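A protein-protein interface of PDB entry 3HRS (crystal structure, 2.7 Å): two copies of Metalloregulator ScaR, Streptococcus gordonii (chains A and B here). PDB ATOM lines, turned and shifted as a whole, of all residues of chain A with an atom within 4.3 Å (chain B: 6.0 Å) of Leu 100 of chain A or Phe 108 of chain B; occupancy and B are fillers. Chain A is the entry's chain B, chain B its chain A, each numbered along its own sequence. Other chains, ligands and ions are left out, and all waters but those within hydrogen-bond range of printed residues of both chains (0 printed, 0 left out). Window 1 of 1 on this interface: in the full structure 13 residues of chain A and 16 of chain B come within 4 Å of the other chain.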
ATOM      1  N   PHE A  81     -13.212  21.214  -8.234  1.00  0.00           N
ATOM      2  CA  PHE A  81     -14.556  20.694  -8.380  1.00  0.00           C
ATOM      3  C   PHE A  81     -15.566  21.481  -7.546  1.00  0.00           C
ATOM      4  O   PHE A  81     -16.536  21.986  -8.103  1.00  0.00           O
ATOM      5  CB  PHE A  81     -14.619  19.195  -8.077  1.00  0.00           C
ATOM      6  CG  PHE A  81     -15.991  18.627  -8.215  1.00  0.00           C
ATOM      7  CD1 PHE A  81     -16.558  18.466  -9.463  1.00  0.00           C
ATOM      8  CD2 PHE A  81     -16.729  18.286  -7.097  1.00  0.00           C
ATOM      9  CE1 PHE A  81     -17.837  17.957  -9.595  1.00  0.00           C
ATOM     10  CE2 PHE A  81     -18.009  17.765  -7.230  1.00  0.00           C
ATOM     11  CZ  PHE A  81     -18.560  17.600  -8.480  1.00  0.00           C
ATOM     12  N   LEU A  82     -15.342  21.597  -6.234  1.00  0.00           N
ATOM     13  CA  LEU A  82     -16.275  22.347  -5.361  1.00  0.00           C
ATOM     14  C   LEU A  82     -16.432  23.817  -5.755  1.00  0.00           C
ATOM     15  O   LEU A  82     -17.530  24.353  -5.697  1.00  0.00           O
ATOM     16  CB  LEU A  82     -15.891  22.255  -3.878  1.00  0.00           C
ATOM     17  CG  LEU A  82     -15.868  20.833  -3.312  1.00  0.00           C
ATOM     18  CD1 LEU A  82     -15.316  20.790  -1.897  1.00  0.00           C
ATOM     19  CD2 LEU A  82     -17.256  20.200  -3.363  1.00  0.00           C
ATOM     20  N   LEU A  86     -19.514  23.057  -8.106  1.00  0.00           N
ATOM     21  CA  LEU A  86     -20.643  23.089  -7.171  1.00  0.00           C
ATOM     22  C   LEU A  86     -20.838  24.503  -6.636  1.00  0.00           C
ATOM     23  O   LEU A  86     -21.645  24.730  -5.731  1.00  0.00           O
ATOM     24  CB  LEU A  86     -20.500  22.060  -6.044  1.00  0.00           C
ATOM     25  CG  LEU A  86     -20.527  20.608  -6.543  1.00  0.00           C
ATOM     26  CD1 LEU A  86     -20.237  19.618  -5.420  1.00  0.00           C
ATOM     27  CD2 LEU A  86     -21.867  20.302  -7.200  1.00  0.00           C
ATOM     28  N   TYR A  88     -19.360  26.327  -4.657  1.00  0.00           N
ATOM     29  CA  TYR A  88     -18.958  26.562  -3.271  1.00  0.00           C
ATOM     30  C   TYR A  88     -18.232  27.889  -3.087  1.00  0.00           C
ATOM     31  O   TYR A  88     -17.503  28.331  -3.977  1.00  0.00           O
ATOM     32  CB  TYR A  88     -18.039  25.437  -2.802  1.00  0.00           C
ATOM     33  CG  TYR A  88     -18.766  24.232  -2.274  1.00  0.00           C
ATOM     34  CD1 TYR A  88     -19.933  23.779  -2.877  1.00  0.00           C
ATOM     35  CD2 TYR A  88     -18.286  23.540  -1.168  1.00  0.00           C
ATOM     36  CE1 TYR A  88     -20.608  22.672  -2.381  1.00  0.00           C
ATOM     37  CE2 TYR A  88     -18.949  22.431  -0.671  1.00  0.00           C
ATOM     38  CZ  TYR A  88     -20.103  21.999  -1.284  1.00  0.00           C
ATOM     39  OH  TYR A  88     -20.759  20.895  -0.797  1.00  0.00           O
ATOM     40  N   GLU A  96     -17.036  21.850   4.416  1.00  0.00           N
ATOM     41  CA  GLU A  96     -17.013  20.454   3.971  1.00  0.00           C
ATOM     42  C   GLU A  96     -15.761  19.951   3.268  1.00  0.00           C
ATOM     43  O   GLU A  96     -15.594  18.741   3.103  1.00  0.00           O
ATOM     44  CB  GLU A  96     -18.255  20.105   3.144  1.00  0.00           C
ATOM     45  CG  GLU A  96     -18.851  21.255   2.369  1.00  0.00           C
ATOM     46  CD  GLU A  96     -20.316  21.025   2.013  1.00  0.00           C
ATOM     47  OE1 GLU A  96     -20.679  19.912   1.543  1.00  0.00           O
ATOM     48  OE2 GLU A  96     -21.106  21.971   2.196  1.00  0.00           O
ATOM     49  N   ALA A  97     -14.886  20.860   2.857  1.00  0.00           N
ATOM     50  CA  ALA A  97     -13.761  20.464   2.011  1.00  0.00           C
ATOM     51  C   ALA A  97     -13.052  19.234   2.554  1.00  0.00           C
ATOM     52  O   ALA A  97     -13.006  18.201   1.894  1.00  0.00           O
ATOM     53  CB  ALA A  97     -12.776  21.610   1.820  1.00  0.00           C
ATOM     54  N   GLU A  98     -12.518  19.330   3.764  1.00  0.00           N
ATOM     55  CA  GLU A  98     -11.596  18.302   4.218  1.00  0.00           C
ATOM     56  C   GLU A  98     -12.232  16.954   4.557  1.00  0.00           C
ATOM     57  O   GLU A  98     -11.539  15.946   4.638  1.00  0.00           O
ATOM     58  CB  GLU A  98     -10.689  18.810   5.348  1.00  0.00           C
ATOM     59  CG  GLU A  98     -11.309  18.847   6.733  1.00  0.00           C
ATOM     60  CD  GLU A  98     -10.322  19.349   7.797  1.00  0.00           C
ATOM     61  OE1 GLU A  98      -9.341  20.042   7.440  1.00  0.00           O
ATOM     62  OE2 GLU A  98     -10.532  19.055   8.994  1.00  0.00           O
ATOM     63  N   VAL A  99     -13.540  16.903   4.744  1.00  0.00           N
ATOM     64  CA  VAL A  99     -14.114  15.609   5.068  1.00  0.00           C
ATOM     65  C   VAL A  99     -14.121  14.747   3.822  1.00  0.00           C
ATOM     66  O   VAL A  99     -13.476  13.701   3.784  1.00  0.00           O
ATOM     67  CB  VAL A  99     -15.516  15.699   5.683  1.00  0.00           C
ATOM     68  CG1 VAL A  99     -15.525  16.747   6.802  1.00  0.00           C
ATOM     69  CG2 VAL A  99     -16.564  16.015   4.606  1.00  0.00           C
ATOM     70  N   LEU A 100     -14.809  15.188   2.783  1.00  0.00           N
ATOM     71  CA  LEU A 100     -14.927  14.313   1.638  1.00  0.00           C
ATOM     72  C   LEU A 100     -13.562  14.175   0.980  1.00  0.00           C
ATOM     73  O   LEU A 100     -13.296  13.226   0.246  1.00  0.00           O
ATOM     74  CB  LEU A 100     -16.042  14.750   0.672  1.00  0.00           C
ATOM     75  CG  LEU A 100     -15.790  15.690  -0.499  1.00  0.00           C
ATOM     76  CD1 LEU A 100     -16.569  15.185  -1.702  1.00  0.00           C
ATOM     77  CD2 LEU A 100     -16.177  17.111  -0.152  1.00  0.00           C
ATOM     78  N   GLU A 101     -12.687  15.113   1.290  1.00  0.00           N
ATOM     79  CA  GLU A 101     -11.300  15.041   0.848  1.00  0.00           C
ATOM     80  C   GLU A 101     -10.570  13.876   1.515  1.00  0.00           C
ATOM     81  O   GLU A 101      -9.638  13.303   0.947  1.00  0.00           O
ATOM     82  CB  GLU A 101     -10.607  16.352   1.176  1.00  0.00           C
ATOM     83  CG  GLU A 101      -9.153  16.367   0.934  1.00  0.00           C
ATOM     84  CD  GLU A 101      -8.572  17.713   1.266  1.00  0.00           C
ATOM     85  OE1 GLU A 101      -9.328  18.703   1.167  1.00  0.00           O
ATOM     86  OE2 GLU A 101      -7.373  17.778   1.623  1.00  0.00           O
ATOM     87  N   HIS A 102     -11.026  13.526   2.713  1.00  0.00           N
ATOM     88  CA  HIS A 102     -10.460  12.439   3.496  1.00  0.00           C
ATOM     89  C   HIS A 102     -11.249  11.139   3.343  1.00  0.00           C
ATOM     90  O   HIS A 102     -10.965  10.157   4.030  1.00  0.00           O
ATOM     91  CB  HIS A 102     -10.417  12.840   4.974  1.00  0.00           C
ATOM     92  CG  HIS A 102      -9.291  13.768   5.315  1.00  0.00           C
ATOM     93  ND1 HIS A 102      -8.450  13.557   6.385  1.00  0.00           N
ATOM     94  CD2 HIS A 102      -8.855  14.902   4.713  1.00  0.00           C
ATOM     95  CE1 HIS A 102      -7.552  14.527   6.438  1.00  0.00           C
ATOM     96  NE2 HIS A 102      -7.777  15.356   5.434  1.00  0.00           N
ATOM     97  N   THR A 103     -12.235  11.130   2.452  1.00  0.00           N
ATOM     98  CA  THR A 103     -13.073   9.951   2.267  1.00  0.00           C
ATOM     99  C   THR A 103     -12.993   9.399   0.857  1.00  0.00           C
ATOM    100  O   THR A 103     -12.948   8.188   0.653  1.00  0.00           O
ATOM    101  CB  THR A 103     -14.526  10.274   2.531  1.00  0.00           C
ATOM    102  OG1 THR A 103     -14.718  10.497   3.930  1.00  0.00           O
ATOM    103  CG2 THR A 103     -15.404   9.126   2.069  1.00  0.00           C
ATOM    104  N   VAL A 104     -12.995  10.298  -0.118  1.00  0.00           N
ATOM    105  CA  VAL A 104     -12.935   9.896  -1.511  1.00  0.00           C
ATOM    106  C   VAL A 104     -11.716   9.038  -1.751  1.00  0.00           C
ATOM    107  O   VAL A 104     -10.646   9.312  -1.223  1.00  0.00           O
ATOM    108  CB  VAL A 104     -12.869  11.101  -2.465  1.00  0.00           C
ATOM    109  CG1 VAL A 104     -14.209  11.821  -2.512  1.00  0.00           C
ATOM    110  CG2 VAL A 104     -11.756  12.031  -2.062  1.00  0.00           C
ATOM    111  N   ILE B  78     -26.044  10.828  -6.217  1.00  0.00           N
ATOM    112  CA  ILE B  78     -24.684  10.305  -6.187  1.00  0.00           C
ATOM    113  C   ILE B  78     -24.561   9.190  -7.231  1.00  0.00           C
ATOM    114  O   ILE B  78     -23.566   9.082  -7.944  1.00  0.00           O
ATOM    115  CB  ILE B  78     -24.289   9.756  -4.794  1.00  0.00           C
ATOM    116  CG1 ILE B  78     -24.293  10.864  -3.726  1.00  0.00           C
ATOM    117  CG2 ILE B  78     -22.921   9.182  -4.825  1.00  0.00           C
ATOM    118  CD1 ILE B  78     -23.604  12.113  -4.179  1.00  0.00           C
ATOM    119  N   PHE B  81     -24.316  10.849 -10.510  1.00  0.00           N
ATOM    120  CA  PHE B  81     -23.035  11.526 -10.680  1.00  0.00           C
ATOM    121  C   PHE B  81     -21.921  10.514 -10.969  1.00  0.00           C
ATOM    122  O   PHE B  81     -21.174  10.685 -11.904  1.00  0.00           O
ATOM    123  CB  PHE B  81     -22.686  12.422  -9.475  1.00  0.00           C
ATOM    124  CG  PHE B  81     -21.279  12.984  -9.506  1.00  0.00           C
ATOM    125  CD1 PHE B  81     -20.958  14.051 -10.334  1.00  0.00           C
ATOM    126  CD2 PHE B  81     -20.283  12.460  -8.682  1.00  0.00           C
ATOM    127  CE1 PHE B  81     -19.659  14.589 -10.339  1.00  0.00           C
ATOM    128  CE2 PHE B  81     -18.983  12.995  -8.674  1.00  0.00           C
ATOM    129  CZ  PHE B  81     -18.669  14.056  -9.500  1.00  0.00           C
ATOM    130  N   THR B 103     -21.575  10.571   4.175  1.00  0.00           N
ATOM    131  CA  THR B 103     -20.549  11.562   4.380  1.00  0.00           C
ATOM    132  C   THR B 103     -20.906  12.919   3.801  1.00  0.00           C
ATOM    133  O   THR B 103     -20.822  13.929   4.492  1.00  0.00           O
ATOM    134  CB  THR B 103     -19.239  11.073   3.770  1.00  0.00           C
ATOM    135  OG1 THR B 103     -18.690  10.059   4.617  1.00  0.00           O
ATOM    136  CG2 THR B 103     -18.231  12.227   3.602  1.00  0.00           C
ATOM    137  N   VAL B 104     -21.286  12.965   2.531  1.00  0.00           N
ATOM    138  CA  VAL B 104     -21.579  14.255   1.931  1.00  0.00           C
ATOM    139  C   VAL B 104     -22.767  14.887   2.621  1.00  0.00           C
ATOM    140  O   VAL B 104     -23.685  14.190   3.090  1.00  0.00           O
ATOM    141  CB  VAL B 104     -21.847  14.175   0.425  1.00  0.00           C
ATOM    142  CG1 VAL B 104     -20.610  13.706  -0.298  1.00  0.00           C
ATOM    143  CG2 VAL B 104     -23.027  13.268   0.153  1.00  0.00           C
ATOM    144  N   SER B 105     -22.716  16.217   2.680  1.00  0.00           N
ATOM    145  CA  SER B 105     -23.748  17.043   3.281  1.00  0.00           C
ATOM    146  C   SER B 105     -24.940  17.249   2.360  1.00  0.00           C
ATOM    147  O   SER B 105     -24.835  17.088   1.142  1.00  0.00           O
ATOM    148  CB  SER B 105     -23.166  18.411   3.592  1.00  0.00           C
ATOM    149  OG  SER B 105     -23.069  19.203   2.422  1.00  0.00           O
ATOM    150  N   ASP B 106     -26.071  17.635   2.933  1.00  0.00           N
ATOM    151  CA  ASP B 106     -27.211  18.007   2.107  1.00  0.00           C
ATOM    152  C   ASP B 106     -26.941  19.175   1.139  1.00  0.00           C
ATOM    153  O   ASP B 106     -27.541  19.257   0.072  1.00  0.00           O
ATOM    154  CB  ASP B 106     -28.439  18.237   2.968  1.00  0.00           C
ATOM    155  CG  ASP B 106     -28.959  16.942   3.566  1.00  0.00           C
ATOM    156  OD1 ASP B 106     -28.413  15.869   3.200  1.00  0.00           O
ATOM    157  OD2 ASP B 106     -29.905  16.993   4.388  1.00  0.00           O
ATOM    158  N   HIS B 107     -26.018  20.055   1.487  1.00  0.00           N
ATOM    159  CA  HIS B 107     -25.689  21.159   0.598  1.00  0.00           C
ATOM    160  C   HIS B 107     -24.895  20.645  -0.620  1.00  0.00           C
ATOM    161  O   HIS B 107     -25.020  21.174  -1.735  1.00  0.00           O
ATOM    162  CB  HIS B 107     -24.916  22.242   1.365  1.00  0.00           C
ATOM    163  CG  HIS B 107     -24.375  23.346   0.504  1.00  0.00           C
ATOM    164  ND1 HIS B 107     -23.023  23.502   0.256  1.00  0.00           N
ATOM    165  CD2 HIS B 107     -24.992  24.372  -0.131  1.00  0.00           C
ATOM    166  CE1 HIS B 107     -22.835  24.562  -0.511  1.00  0.00           C
ATOM    167  NE2 HIS B 107     -24.014  25.111  -0.759  1.00  0.00           N
ATOM    168  N   PHE B 108     -24.069  19.628  -0.397  1.00  0.00           N
ATOM    169  CA  PHE B 108     -23.377  18.977  -1.496  1.00  0.00           C
ATOM    170  C   PHE B 108     -24.454  18.420  -2.426  1.00  0.00           C
ATOM    171  O   PHE B 108     -24.440  18.641  -3.624  1.00  0.00           O
ATOM    172  CB  PHE B 108     -22.476  17.844  -0.976  1.00  0.00           C
ATOM    173  CG  PHE B 108     -21.682  17.155  -2.054  1.00  0.00           C
ATOM    174  CD1 PHE B 108     -20.395  17.601  -2.390  1.00  0.00           C
ATOM    175  CD2 PHE B 108     -22.215  16.065  -2.743  1.00  0.00           C
ATOM    176  CE1 PHE B 108     -19.647  16.966  -3.391  1.00  0.00           C
ATOM    177  CE2 PHE B 108     -21.479  15.419  -3.757  1.00  0.00           C
ATOM    178  CZ  PHE B 108     -20.195  15.868  -4.078  1.00  0.00           C
ATOM    179  N   VAL B 109     -25.414  17.718  -1.852  1.00  0.00           N
ATOM    180  CA  VAL B 109     -26.415  17.072  -2.660  1.00  0.00           C
ATOM    181  C   VAL B 109     -27.217  18.099  -3.438  1.00  0.00           C
ATOM    182  O   VAL B 109     -27.519  17.897  -4.602  1.00  0.00           O
ATOM    183  CB  VAL B 109     -27.293  16.141  -1.816  1.00  0.00           C
ATOM    184  CG1 VAL B 109     -28.364  15.499  -2.649  1.00  0.00           C
ATOM    185  CG2 VAL B 109     -26.424  15.060  -1.205  1.00  0.00           C
ATOM    186  N   GLU B 110     -27.515  19.230  -2.830  1.00  0.00           N
ATOM    187  CA  GLU B 110     -28.256  20.249  -3.564  1.00  0.00           C
ATOM    188  C   GLU B 110     -27.442  20.815  -4.718  1.00  0.00           C
ATOM    189  O   GLU B 110     -27.950  20.940  -5.825  1.00  0.00           O
ATOM    190  CB  GLU B 110     -28.767  21.361  -2.648  1.00  0.00           C
ATOM    191  CG  GLU B 110     -30.280  21.374  -2.503  1.00  0.00           C
ATOM    192  CD  GLU B 110     -30.860  20.006  -2.137  1.00  0.00           C
ATOM    193  OE1 GLU B 110     -30.280  19.290  -1.289  1.00  0.00           O
ATOM    194  OE2 GLU B 110     -31.917  19.651  -2.693  1.00  0.00           O
ATOM    195  N   ARG B 111     -26.180  21.144  -4.478  1.00  0.00           N
ATOM    196  CA  ARG B 111     -25.359  21.666  -5.573  1.00  0.00           C
ATOM    197  C   ARG B 111     -25.218  20.613  -6.697  1.00  0.00           C
ATOM    198  O   ARG B 111     -25.401  20.920  -7.881  1.00  0.00           O
ATOM    199  CB  ARG B 111     -23.994  22.115  -5.054  1.00  0.00           C
ATOM    200  CG  ARG B 111     -24.060  23.095  -3.881  1.00  0.00           C
ATOM    201  CD  ARG B 111     -24.963  24.261  -4.183  1.00  0.00           C
ATOM    202  NE  ARG B 111     -24.590  24.892  -5.438  1.00  0.00           N
ATOM    203  CZ  ARG B 111     -25.093  26.039  -5.885  1.00  0.00           C
ATOM    204  NH1 ARG B 111     -25.998  26.702  -5.169  1.00  0.00           N
ATOM    205  NH2 ARG B 111     -24.681  26.529  -7.050  1.00  0.00           N
ATOM    206  N   LEU B 112     -24.908  19.380  -6.289  1.00  0.00           N
ATOM    207  CA  LEU B 112     -24.819  18.233  -7.163  1.00  0.00           C
ATOM    208  C   LEU B 112     -26.007  18.178  -8.092  1.00  0.00           C
ATOM    209  O   LEU B 112     -25.858  17.953  -9.279  1.00  0.00           O
ATOM    210  CB  LEU B 112     -24.806  16.953  -6.342  1.00  0.00           C
ATOM    211  CG  LEU B 112     -23.839  15.854  -6.785  1.00  0.00           C
ATOM    212  CD1 LEU B 112     -24.567  14.543  -6.765  1.00  0.00           C
ATOM    213  CD2 LEU B 112     -23.198  16.127  -8.174  1.00  0.00           C
ATOM    214  N   ASP B 113     -27.193  18.364  -7.531  1.00  0.00           N
ATOM    215  CA  ASP B 113     -28.432  18.262  -8.296  1.00  0.00           C
ATOM    216  C   ASP B 113     -28.382  19.247  -9.438  1.00  0.00           C
ATOM    217  O   ASP B 113     -28.686  18.917 -10.571  1.00  0.00           O
ATOM    218  CB  ASP B 113     -29.629  18.582  -7.397  1.00  0.00           C
ATOM    219  CG  ASP B 113     -30.961  18.210  -8.024  1.00  0.00           C
ATOM    220  OD1 ASP B 113     -31.015  17.329  -8.907  1.00  0.00           O
ATOM    221  OD2 ASP B 113     -31.973  18.799  -7.606  1.00  0.00           O
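Leu 100 of chain A touches just one residue of chain B: Phe 108.
Of chain A, only Leu 86 (3.4 Å), Tyr 88 (3.3 Å), Glu 96 (3.7 Å) and Leu 100 (3.9 Å) come within 4 Å of Phe 108 of chain B.
Of the printed residues of chain A, Ser 105 of chain B touches Glu 96.
Printed residues of chain A within 4 Å of Arg 111 of chain B: Leu 86 and Tyr 88.
The nearest residue of chain A that does not touch Phe 108 of chain B is Leu 82 of chain A (4.02 Å).
Phe 81 of chain B touches its own counterpart, Phe 81 of chain A.
Thr 103 of chain B touches its own counterpart, Thr 103 of chain A.
Positions printed for both chains: 81, 103 and 104.
Hydrophobic or aromatic side chains of chain A within 4 Å of the printed part of chain B: Phe 81, Leu 86, Tyr 88 and Leu 100.
Hydrophobic or aromatic side chains of chain B within 4 Å of the printed part of chain A: Phe 81, His 107 and Phe 108.
Among the printed residues, 12 pairs touch across the chains.
Among the printed residues, no Asp or Glu carboxylate lies within 4 Å of a Lys or Arg side-chain nitrogen of the other chain.
The side-chain hydroxyl (OG) of Ser 105 of chain B is in hydrogen-bond range of the side-chain carboxylate (OE1) of Glu 96 of chain A, 2.6 Å away.
ND1 of His 107 of chain B is in hydrogen-bond range of OE2 of Glu 96 of chain A, at 3.1 Å.
NE of Arg 111 of chain B lies within hydrogen-bond range of O of Leu 86 of chain A (3.0 Å).
Phe 81 of chain A touches Phe 81 of chain B.
Phe 108 of chain B touches Leu 86 of chain A (CE1 to CD1, 3.4 Å).
Leu 86 of chain A touches Leu 112 of chain B.
Tyr 88 of chain A touches His 107 of chain B (CE1 to CE1, 3.5 Å).
Tyr 88 of chain A touches Phe 108 of chain B (OH to CA, 3.3 Å).
Tyr 88 of chain A touches Arg 111 of chain B (CE1 to CG, 3.8 Å).
OE1 of Glu 96 of chain A touches CB of Phe 108 of chain B (3.7 Å).
Leu 100 of chain A touches Phe 108 of chain B.
Thr 103 of chain A touches Thr 103 of chain B.
The backbone carbonyl oxygen (O) of Val 99 of chain A is in hydrogen-bond range of the side-chain hydroxyl (OG1) of Thr 103 of chain A (3.4 Å).
The backbone NH of Tyr 88 of chain A sits at hydrogen-bond distance from the backbone carbonyl oxygen of Leu 82 of chain A (2.9 Å).
The side-chain hydroxyl (OG) of Ser 105 of chain B lies close to the backbone NH (N) of His 107 of chain B (3.2 Å).
OG of Ser 105 of chain B sits at hydrogen-bond distance from N of Phe 108 of chain B (3.0 Å).
The backbone NH (N) of Leu 86 of chain A is in hydrogen-bond range of the backbone carbonyl oxygen (O) of Phe 81 of chain A (3.2 Å).
The side-chain carboxylate (OE1) of Glu 96 of chain A sits at hydrogen-bond distance from the side-chain hydroxyl (OH) of Tyr 88 of chain A.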
